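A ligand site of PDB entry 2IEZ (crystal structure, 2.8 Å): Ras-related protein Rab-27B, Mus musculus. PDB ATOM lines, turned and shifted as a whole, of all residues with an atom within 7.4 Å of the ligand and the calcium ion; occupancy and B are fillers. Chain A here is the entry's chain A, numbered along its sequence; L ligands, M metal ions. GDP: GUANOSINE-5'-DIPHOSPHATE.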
ATOM      1  N   ALA A  16     -28.563  25.957 -11.308  1.00  0.00           N
ATOM      2  CA  ALA A  16     -27.619  25.464 -12.331  1.00  0.00           C
ATOM      3  C   ALA A  16     -26.298  26.212 -12.243  1.00  0.00           C
ATOM      4  O   ALA A  16     -26.218  27.392 -12.595  1.00  0.00           O
ATOM      5  CB  ALA A  16     -28.217  25.547 -13.731  1.00  0.00           C
ATOM      6  N   LEU A  17     -25.252  25.524 -11.779  1.00  0.00           N
ATOM      7  CA  LEU A  17     -23.957  26.130 -11.515  1.00  0.00           C
ATOM      8  C   LEU A  17     -22.869  25.629 -12.470  1.00  0.00           C
ATOM      9  O   LEU A  17     -23.033  24.601 -13.107  1.00  0.00           O
ATOM     10  CB  LEU A  17     -23.542  25.898 -10.055  1.00  0.00           C
ATOM     11  CG  LEU A  17     -24.374  26.573  -8.953  1.00  0.00           C
ATOM     12  CD1 LEU A  17     -24.110  25.905  -7.630  1.00  0.00           C
ATOM     13  CD2 LEU A  17     -24.059  28.060  -8.863  1.00  0.00           C
ATOM     14  N   GLY A  18     -21.763  26.373 -12.548  1.00  0.00           N
ATOM     15  CA  GLY A  18     -20.673  26.055 -13.478  1.00  0.00           C
ATOM     16  C   GLY A  18     -20.251  27.277 -14.285  1.00  0.00           C
ATOM     17  O   GLY A  18     -21.023  28.223 -14.438  1.00  0.00           O
ATOM     18  N   ASP A  19     -19.024  27.245 -14.807  1.00  0.00           N
ATOM     19  CA  ASP A  19     -18.469  28.382 -15.562  1.00  0.00           C
ATOM     20  C   ASP A  19     -19.107  28.510 -16.947  1.00  0.00           C
ATOM     21  O   ASP A  19     -19.582  27.511 -17.506  1.00  0.00           O
ATOM     22  CB  ASP A  19     -16.947  28.299 -15.650  1.00  0.00           C
ATOM     23  CG  ASP A  19     -16.259  28.502 -14.297  1.00  0.00           C
ATOM     24  OD1 ASP A  19     -16.494  27.685 -13.386  1.00  0.00           O
ATOM     25  OD2 ASP A  19     -15.496  29.474 -14.138  1.00  0.00           O
ATOM     26  N   SER A  20     -19.120  29.733 -17.486  1.00  0.00           N
ATOM     27  CA  SER A  20     -19.847  30.049 -18.719  1.00  0.00           C
ATOM     28  C   SER A  20     -19.463  29.191 -19.929  1.00  0.00           C
ATOM     29  O   SER A  20     -18.330  28.691 -20.040  1.00  0.00           O
ATOM     30  CB  SER A  20     -19.669  31.519 -19.089  1.00  0.00           C
ATOM     31  OG  SER A  20     -19.741  32.327 -17.935  1.00  0.00           O
ATOM     32  N   GLY A  21     -20.437  29.026 -20.840  1.00  0.00           N
ATOM     33  CA  GLY A  21     -20.246  28.265 -22.061  1.00  0.00           C
ATOM     34  C   GLY A  21     -20.310  26.775 -21.843  1.00  0.00           C
ATOM     35  O   GLY A  21     -20.239  26.008 -22.792  1.00  0.00           O
ATOM     36  N   VAL A  22     -20.454  26.360 -20.589  1.00  0.00           N
ATOM     37  CA  VAL A  22     -20.544  24.940 -20.243  1.00  0.00           C
ATOM     38  C   VAL A  22     -21.878  24.315 -20.635  1.00  0.00           C
ATOM     39  O   VAL A  22     -21.969  23.087 -20.762  1.00  0.00           O
ATOM     40  CB  VAL A  22     -20.216  24.700 -18.746  1.00  0.00           C
ATOM     41  CG1 VAL A  22     -20.944  23.494 -18.187  1.00  0.00           C
ATOM     42  CG2 VAL A  22     -18.725  24.566 -18.549  1.00  0.00           C
ATOM     43  N   GLY A  23     -22.908  25.142 -20.834  1.00  0.00           N
ATOM     44  CA  GLY A  23     -24.179  24.698 -21.411  1.00  0.00           C
ATOM     45  C   GLY A  23     -25.385  24.569 -20.485  1.00  0.00           C
ATOM     46  O   GLY A  23     -26.317  23.812 -20.772  1.00  0.00           O
ATOM     47  N   LYS A  24     -25.390  25.311 -19.382  1.00  0.00           N
ATOM     48  CA  LYS A  24     -26.484  25.215 -18.420  1.00  0.00           C
ATOM     49  C   LYS A  24     -27.798  25.786 -18.926  1.00  0.00           C
ATOM     50  O   LYS A  24     -28.847  25.191 -18.709  1.00  0.00           O
ATOM     51  CB  LYS A  24     -26.114  25.806 -17.061  1.00  0.00           C
ATOM     52  CG  LYS A  24     -25.227  27.038 -17.079  1.00  0.00           C
ATOM     53  CD  LYS A  24     -24.607  27.237 -15.700  1.00  0.00           C
ATOM     54  CE  LYS A  24     -24.118  28.649 -15.495  1.00  0.00           C
ATOM     55  NZ  LYS A  24     -23.015  28.991 -16.419  1.00  0.00           N
ATOM     56  N   THR A  25     -27.739  26.915 -19.634  1.00  0.00           N
ATOM     57  CA  THR A  25     -28.945  27.493 -20.219  1.00  0.00           C
ATOM     58  C   THR A  25     -29.520  26.505 -21.242  1.00  0.00           C
ATOM     59  O   THR A  25     -30.718  26.219 -21.231  1.00  0.00           O
ATOM     60  CB  THR A  25     -28.672  28.859 -20.902  1.00  0.00           C
ATOM     61  OG1 THR A  25     -27.920  29.706 -20.015  1.00  0.00           O
ATOM     62  CG2 THR A  25     -29.974  29.537 -21.289  1.00  0.00           C
ATOM     63  N   THR A  26     -28.664  25.990 -22.104  1.00  0.00           N
ATOM     64  CA  THR A  26     -29.080  24.986 -23.071  1.00  0.00           C
ATOM     65  C   THR A  26     -29.679  23.802 -22.324  1.00  0.00           C
ATOM     66  O   THR A  26     -30.833  23.444 -22.529  1.00  0.00           O
ATOM     67  CB  THR A  26     -27.897  24.542 -23.949  1.00  0.00           C
ATOM     68  OG1 THR A  26     -27.139  25.694 -24.350  1.00  0.00           O
ATOM     69  CG2 THR A  26     -28.379  23.810 -25.182  1.00  0.00           C
ATOM     70  N   PHE A  27     -28.881  23.207 -21.437  1.00  0.00           N
ATOM     71  CA  PHE A  27     -29.295  22.120 -20.547  1.00  0.00           C
ATOM     72  C   PHE A  27     -30.700  22.285 -19.967  1.00  0.00           C
ATOM     73  O   PHE A  27     -31.457  21.331 -19.877  1.00  0.00           O
ATOM     74  CB  PHE A  27     -28.270  21.982 -19.408  1.00  0.00           C
ATOM     75  CG  PHE A  27     -28.412  20.724 -18.593  1.00  0.00           C
ATOM     76  CD1 PHE A  27     -27.703  19.578 -18.952  1.00  0.00           C
ATOM     77  CD2 PHE A  27     -29.229  20.684 -17.467  1.00  0.00           C
ATOM     78  CE1 PHE A  27     -27.826  18.404 -18.210  1.00  0.00           C
ATOM     79  CE2 PHE A  27     -29.358  19.525 -16.718  1.00  0.00           C
ATOM     80  CZ  PHE A  27     -28.652  18.375 -17.086  1.00  0.00           C
ATOM     81  N   LEU A  28     -31.041  23.504 -19.592  1.00  0.00           N
ATOM     82  CA  LEU A  28     -32.349  23.770 -19.003  1.00  0.00           C
ATOM     83  C   LEU A  28     -33.444  23.935 -20.035  1.00  0.00           C
ATOM     84  O   LEU A  28     -34.560  23.448 -19.836  1.00  0.00           O
ATOM     85  CB  LEU A  28     -32.288  24.994 -18.073  1.00  0.00           C
ATOM     86  CG  LEU A  28     -31.393  24.864 -16.830  1.00  0.00           C
ATOM     87  CD1 LEU A  28     -31.398  26.152 -16.002  1.00  0.00           C
ATOM     88  CD2 LEU A  28     -31.786  23.666 -15.975  1.00  0.00           C
ATOM     89  N   ARG A  30     -34.152  22.664 -23.238  1.00  0.00           N
ATOM     90  CA  ARG A  30     -34.769  21.478 -23.827  1.00  0.00           C
ATOM     91  C   ARG A  30     -35.403  20.563 -22.789  1.00  0.00           C
ATOM     92  O   ARG A  30     -36.415  19.919 -23.067  1.00  0.00           O
ATOM     93  CB  ARG A  30     -33.780  20.686 -24.681  1.00  0.00           C
ATOM     94  CG  ARG A  30     -33.301  21.431 -25.930  1.00  0.00           C
ATOM     95  CD  ARG A  30     -32.187  20.689 -26.632  1.00  0.00           C
ATOM     96  NE  ARG A  30     -31.324  21.596 -27.397  1.00  0.00           N
ATOM     97  CZ  ARG A  30     -30.416  21.203 -28.280  1.00  0.00           C
ATOM     98  NH1 ARG A  30     -30.254  19.905 -28.548  1.00  0.00           N
ATOM     99  NH2 ARG A  30     -29.669  22.097 -28.913  1.00  0.00           N
ATOM    100  N   MET A 100     -22.283  21.373 -12.942  1.00  0.00           N
ATOM    101  CA  MET A 100     -21.736  20.913 -14.211  1.00  0.00           C
ATOM    102  C   MET A 100     -20.430  21.600 -14.606  1.00  0.00           C
ATOM    103  O   MET A 100     -20.158  22.743 -14.209  1.00  0.00           O
ATOM    104  CB  MET A 100     -22.771  21.026 -15.334  1.00  0.00           C
ATOM    105  CG  MET A 100     -23.646  22.273 -15.318  1.00  0.00           C
ATOM    106  SD  MET A 100     -24.932  22.289 -16.593  1.00  0.00           S
ATOM    107  CE  MET A 100     -25.754  20.735 -16.273  1.00  0.00           C
ATOM    108  N   ASP A 102     -17.384  21.325 -18.137  1.00  0.00           N
ATOM    109  CA  ASP A 102     -17.262  20.900 -19.525  1.00  0.00           C
ATOM    110  C   ASP A 102     -16.369  19.659 -19.634  1.00  0.00           C
ATOM    111  O   ASP A 102     -15.296  19.606 -19.016  1.00  0.00           O
ATOM    112  CB  ASP A 102     -16.729  22.033 -20.400  1.00  0.00           C
ATOM    113  CG  ASP A 102     -17.181  21.921 -21.850  1.00  0.00           C
ATOM    114  OD1 ASP A 102     -17.849  20.927 -22.187  1.00  0.00           O
ATOM    115  OD2 ASP A 102     -16.865  22.835 -22.652  1.00  0.00           O
ATOM    116  N   GLY A 134     -21.256  16.300 -15.950  1.00  0.00           N
ATOM    117  CA  GLY A 134     -20.296  16.551 -17.023  1.00  0.00           C
ATOM    118  C   GLY A 134     -21.026  16.645 -18.333  1.00  0.00           C
ATOM    119  O   GLY A 134     -21.547  15.648 -18.829  1.00  0.00           O
ATOM    120  N   ASN A 135     -21.096  17.866 -18.885  1.00  0.00           N
ATOM    121  CA  ASN A 135     -21.839  18.112 -20.124  1.00  0.00           C
ATOM    122  C   ASN A 135     -20.968  18.021 -21.382  1.00  0.00           C
ATOM    123  O   ASN A 135     -19.738  17.976 -21.286  1.00  0.00           O
ATOM    124  CB  ASN A 135     -22.564  19.463 -20.063  1.00  0.00           C
ATOM    125  CG  ASN A 135     -23.613  19.625 -21.158  1.00  0.00           C
ATOM    126  OD1 ASN A 135     -24.541  18.801 -21.295  1.00  0.00           O
ATOM    127  ND2 ASN A 135     -23.492  20.689 -21.938  1.00  0.00           N
ATOM    128  N   LYS A 136     -21.617  18.010 -22.538  1.00  0.00           N
ATOM    129  CA  LYS A 136     -20.941  17.852 -23.842  1.00  0.00           C
ATOM    130  C   LYS A 136     -20.211  16.508 -23.887  1.00  0.00           C
ATOM    131  O   LYS A 136     -18.986  16.438 -23.752  1.00  0.00           O
ATOM    132  CB  LYS A 136     -20.001  19.020 -24.167  1.00  0.00           C
ATOM    133  CG  LYS A 136     -20.653  20.396 -24.050  1.00  0.00           C
ATOM    134  CD  LYS A 136     -19.763  21.522 -24.570  1.00  0.00           C
ATOM    135  CE  LYS A 136     -20.470  22.867 -24.476  1.00  0.00           C
ATOM    136  NZ  LYS A 136     -19.643  23.996 -24.998  1.00  0.00           N
ATOM    137  N   ALA A 137     -20.986  15.434 -24.049  1.00  0.00           N
ATOM    138  CA  ALA A 137     -20.464  14.075 -24.149  1.00  0.00           C
ATOM    139  C   ALA A 137     -20.736  13.564 -25.560  1.00  0.00           C
ATOM    140  O   ALA A 137     -20.358  12.452 -25.920  1.00  0.00           O
ATOM    141  CB  ALA A 137     -21.119  13.184 -23.091  1.00  0.00           C
ATOM    142  N   ASP A 138     -21.419  14.405 -26.330  1.00  0.00           N
ATOM    143  CA  ASP A 138     -21.709  14.148 -27.733  1.00  0.00           C
ATOM    144  C   ASP A 138     -20.510  14.610 -28.588  1.00  0.00           C
ATOM    145  O   ASP A 138     -20.562  14.572 -29.824  1.00  0.00           O
ATOM    146  CB  ASP A 138     -22.969  14.903 -28.140  1.00  0.00           C
ATOM    147  CG  ASP A 138     -22.857  16.401 -27.909  1.00  0.00           C
ATOM    148  OD1 ASP A 138     -22.709  16.827 -26.739  1.00  0.00           O
ATOM    149  OD2 ASP A 138     -22.892  17.154 -28.911  1.00  0.00           O
ATOM    150  N   LEU A 139     -19.451  15.036 -27.923  1.00  0.00           N
ATOM    151  CA  LEU A 139     -18.227  15.465 -28.582  1.00  0.00           C
ATOM    152  C   LEU A 139     -17.030  14.838 -27.874  1.00  0.00           C
ATOM    153  O   LEU A 139     -16.277  15.536 -27.184  1.00  0.00           O
ATOM    154  CB  LEU A 139     -18.113  16.988 -28.600  1.00  0.00           C
ATOM    155  CG  LEU A 139     -19.127  17.779 -29.423  1.00  0.00           C
ATOM    156  CD1 LEU A 139     -18.942  19.280 -29.197  1.00  0.00           C
ATOM    157  CD2 LEU A 139     -19.070  17.445 -30.927  1.00  0.00           C
ATOM    158  N   THR A 164     -23.528  13.794 -19.294  1.00  0.00           N
ATOM    159  CA  THR A 164     -24.713  14.334 -19.927  1.00  0.00           C
ATOM    160  C   THR A 164     -24.349  15.126 -21.169  1.00  0.00           C
ATOM    161  O   THR A 164     -23.198  15.514 -21.356  1.00  0.00           O
ATOM    162  CB  THR A 164     -25.510  15.225 -18.946  1.00  0.00           C
ATOM    163  OG1 THR A 164     -26.849  15.409 -19.438  1.00  0.00           O
ATOM    164  CG2 THR A 164     -24.834  16.580 -18.782  1.00  0.00           C
ATOM    165  N   SER A 165     -25.349  15.328 -22.031  1.00  0.00           N
ATOM    166  CA  SER A 165     -25.225  16.189 -23.194  1.00  0.00           C
ATOM    167  C   SER A 165     -26.576  16.826 -23.496  1.00  0.00           C
ATOM    168  O   SER A 165     -27.540  16.126 -23.788  1.00  0.00           O
ATOM    169  CB  SER A 165     -24.696  15.421 -24.408  1.00  0.00           C
ATOM    170  OG  SER A 165     -25.681  14.581 -24.988  1.00  0.00           O
ATOM    171  N   ALA A 166     -26.634  18.155 -23.411  1.00  0.00           N
ATOM    172  CA  ALA A 166     -27.874  18.871 -23.676  1.00  0.00           C
ATOM    173  C   ALA A 166     -28.267  18.837 -25.164  1.00  0.00           C
ATOM    174  O   ALA A 166     -29.365  19.252 -25.531  1.00  0.00           O
ATOM    175  CB  ALA A 166     -27.761  20.301 -23.187  1.00  0.00           C
ATOM    176  N   ALA A 167     -27.362  18.314 -25.993  1.00  0.00           N
ATOM    177  CA  ALA A 167     -27.594  18.172 -27.427  1.00  0.00           C
ATOM    178  C   ALA A 167     -28.390  16.917 -27.762  1.00  0.00           C
ATOM    179  O   ALA A 167     -29.441  17.001 -28.404  1.00  0.00           O
ATOM    180  CB  ALA A 167     -26.273  18.180 -28.182  1.00  0.00           C
ATOM    181  N   THR A 168     -27.885  15.760 -27.333  1.00  0.00           N
ATOM    182  CA  THR A 168     -28.571  14.487 -27.558  1.00  0.00           C
ATOM    183  C   THR A 168     -29.730  14.314 -26.579  1.00  0.00           C
ATOM    184  O   THR A 168     -30.704  13.616 -26.869  1.00  0.00           O
ATOM    185  CB  THR A 168     -27.597  13.279 -27.466  1.00  0.00           C
ATOM    186  OG1 THR A 168     -26.508  13.474 -28.369  1.00  0.00           O
ATOM    187  CG2 THR A 168     -28.299  11.971 -27.844  1.00  0.00           C
ATOM    188  N   GLY A 169     -29.630  14.969 -25.413  1.00  0.00           N
ATOM    189  CA  GLY A 169     -30.602  14.804 -24.331  1.00  0.00           C
ATOM    190  C   GLY A 169     -30.153  13.715 -23.373  1.00  0.00           C
ATOM    191  O   GLY A 169     -30.886  13.364 -22.440  1.00  0.00           O
HETATM  192  PB  GDP L   1     -23.998  28.637 -20.346  1.00  0.00           P
HETATM  193  O1B GDP L   1     -23.780  30.139 -20.392  1.00  0.00           O
HETATM  194  O2B GDP L   1     -23.148  28.003 -19.270  1.00  0.00           O
HETATM  195  O3B GDP L   1     -25.438  28.386 -20.003  1.00  0.00           O
HETATM  196  O3A GDP L   1     -23.642  27.954 -21.763  1.00  0.00           O
HETATM  197  PA  GDP L   1     -24.689  27.920 -22.972  1.00  0.00           P
HETATM  198  O1A GDP L   1     -25.924  27.111 -22.648  1.00  0.00           O
HETATM  199  O2A GDP L   1     -25.089  29.328 -23.319  1.00  0.00           O
HETATM  200  O5' GDP L   1     -23.853  27.232 -24.164  1.00  0.00           O
HETATM  201  C5' GDP L   1     -23.377  28.016 -25.254  1.00  0.00           C
HETATM  202  C4' GDP L   1     -23.184  27.149 -26.506  1.00  0.00           C
HETATM  203  O4' GDP L   1     -22.678  25.863 -26.129  1.00  0.00           O
HETATM  204  C3' GDP L   1     -24.492  26.938 -27.246  1.00  0.00           C
HETATM  205  O3' GDP L   1     -24.488  27.637 -28.496  1.00  0.00           O
HETATM  206  C2' GDP L   1     -24.611  25.439 -27.462  1.00  0.00           C
HETATM  207  O2' GDP L   1     -24.743  25.119 -28.856  1.00  0.00           O
HETATM  208  C1' GDP L   1     -23.312  24.854 -26.920  1.00  0.00           C
HETATM  209  N9  GDP L   1     -23.577  23.667 -26.070  1.00  0.00           N
HETATM  210  C8  GDP L   1     -24.075  23.691 -24.824  1.00  0.00           C
HETATM  211  N7  GDP L   1     -24.192  22.429 -24.311  1.00  0.00           N
HETATM  212  C5  GDP L   1     -23.770  21.578 -25.266  1.00  0.00           C
HETATM  213  C6  GDP L   1     -23.627  20.107 -25.394  1.00  0.00           C
HETATM  214  O6  GDP L   1     -23.948  19.345 -24.454  1.00  0.00           O
HETATM  215  N1  GDP L   1     -23.147  19.624 -26.544  1.00  0.00           N
HETATM  216  C2  GDP L   1     -22.790  20.416 -27.571  1.00  0.00           C
HETATM  217  N2  GDP L   1     -22.322  19.855 -28.701  1.00  0.00           N
HETATM  218  N3  GDP L   1     -22.896  21.772 -27.529  1.00  0.00           N
HETATM  219  C4  GDP L   1     -23.366  22.401 -26.421  1.00  0.00           C
HETATM  220 CA    CA M   1     -25.964  30.690 -21.178  1.00  0.00          CA
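The backbone NH (N) of Thr 25 sits close to an oxygen (O3B) of the ligand, 2.8 Å away.
N of Thr 26 lies within hydrogen-bond range of O1A of the ligand.
OG1 of Thr 26 sits at hydrogen-bond distance from O1A of the ligand, at 2.5 Å.
OD2 of Asp 138 is in hydrogen-bond range of N2 of the ligand (2.8 Å).
O6 of the ligand sits at hydrogen-bond distance from ND2 of Asn 135.
O3B of the ligand sits close to N of Lys 24 (3.1 Å).
The side-chain amino group (NZ) of Lys 24 lies within salt-bridge range of an oxygen (O2B) of the ligand, at 3.0 Å.
The backbone NH of Gly 23 sits at hydrogen-bond distance from an oxygen (O3A) of the ligand (3.1 Å).
O6 of the ligand sits at hydrogen-bond distance from N of Ala 166.
The backbone NH (N) of Lys 136 lies within hydrogen-bond range of an oxygen (O6) of the ligand (3.3 Å).
N of Gly 21 is in hydrogen-bond range of O2B of the ligand, at 3.3 Å.
N of Val 22 lies within hydrogen-bond range of O2B of the ligand, 3.4 Å away.
The side-chain amide oxygen (OD1) of Asn 135 is in hydrogen-bond range of the backbone NH (N) of Ala 166.
ND2 of Asn 135 lies within hydrogen-bond range of O of Val 22, at 3.1 Å.
NZ of Lys 24 lies within hydrogen-bond range of O of Gly 18 (2.9 Å).
The guanidinium group (NH1) of Arg 30 is in hydrogen-bond range of the backbone carbonyl oxygen (O) of Ala 166.
The backbone carbonyl oxygen (O) of Gly 21 lies within hydrogen-bond range of the side-chain amino group (NZ) of Lys 136 (3.0 Å).
N of Lys 136 sits at hydrogen-bond distance from O of Thr 164.
The side-chain hydroxyl (OG) of Ser 165 lies close to the backbone NH (N) of Thr 168, at 3.4 Å.
The guanidinium group (NH1) of Arg 30 is in hydrogen-bond range of the backbone carbonyl oxygen (O) of Ala 167, 3.0 Å away.
Ser 20 touches the ligand (CA to O2B, 3.9 Å).
CD1 of Leu 139 touches N2 of the ligand (3.5 Å).
Ser 165 touches the ligand.
Ala 167 touches the ligand.
Hydrophobic or aromatic side chains within 4 Å of the ligand: Leu 139 and Ala 167.
Within 4 Å of the ligand: Ser 20, Gly 21, Val 22, Gly 23, Lys 24, Thr 25, Thr 26, Asn 135, Lys 136, Asp 138, Leu 139, Ser 165, Ala 166 and Ala 167.
The nearest printed residue that does not touch the ligand is Asp 19 (4.01 Å).
The calcium ion is bound by an oxygen (O1B) of the ligand (2.4 Å), the side-chain hydroxyl (OG1) of Thr 25 (2.5 Å), an oxygen (O3B) of the ligand (2.6 Å) and an oxygen (O2A) of the ligand (2.7 Å).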
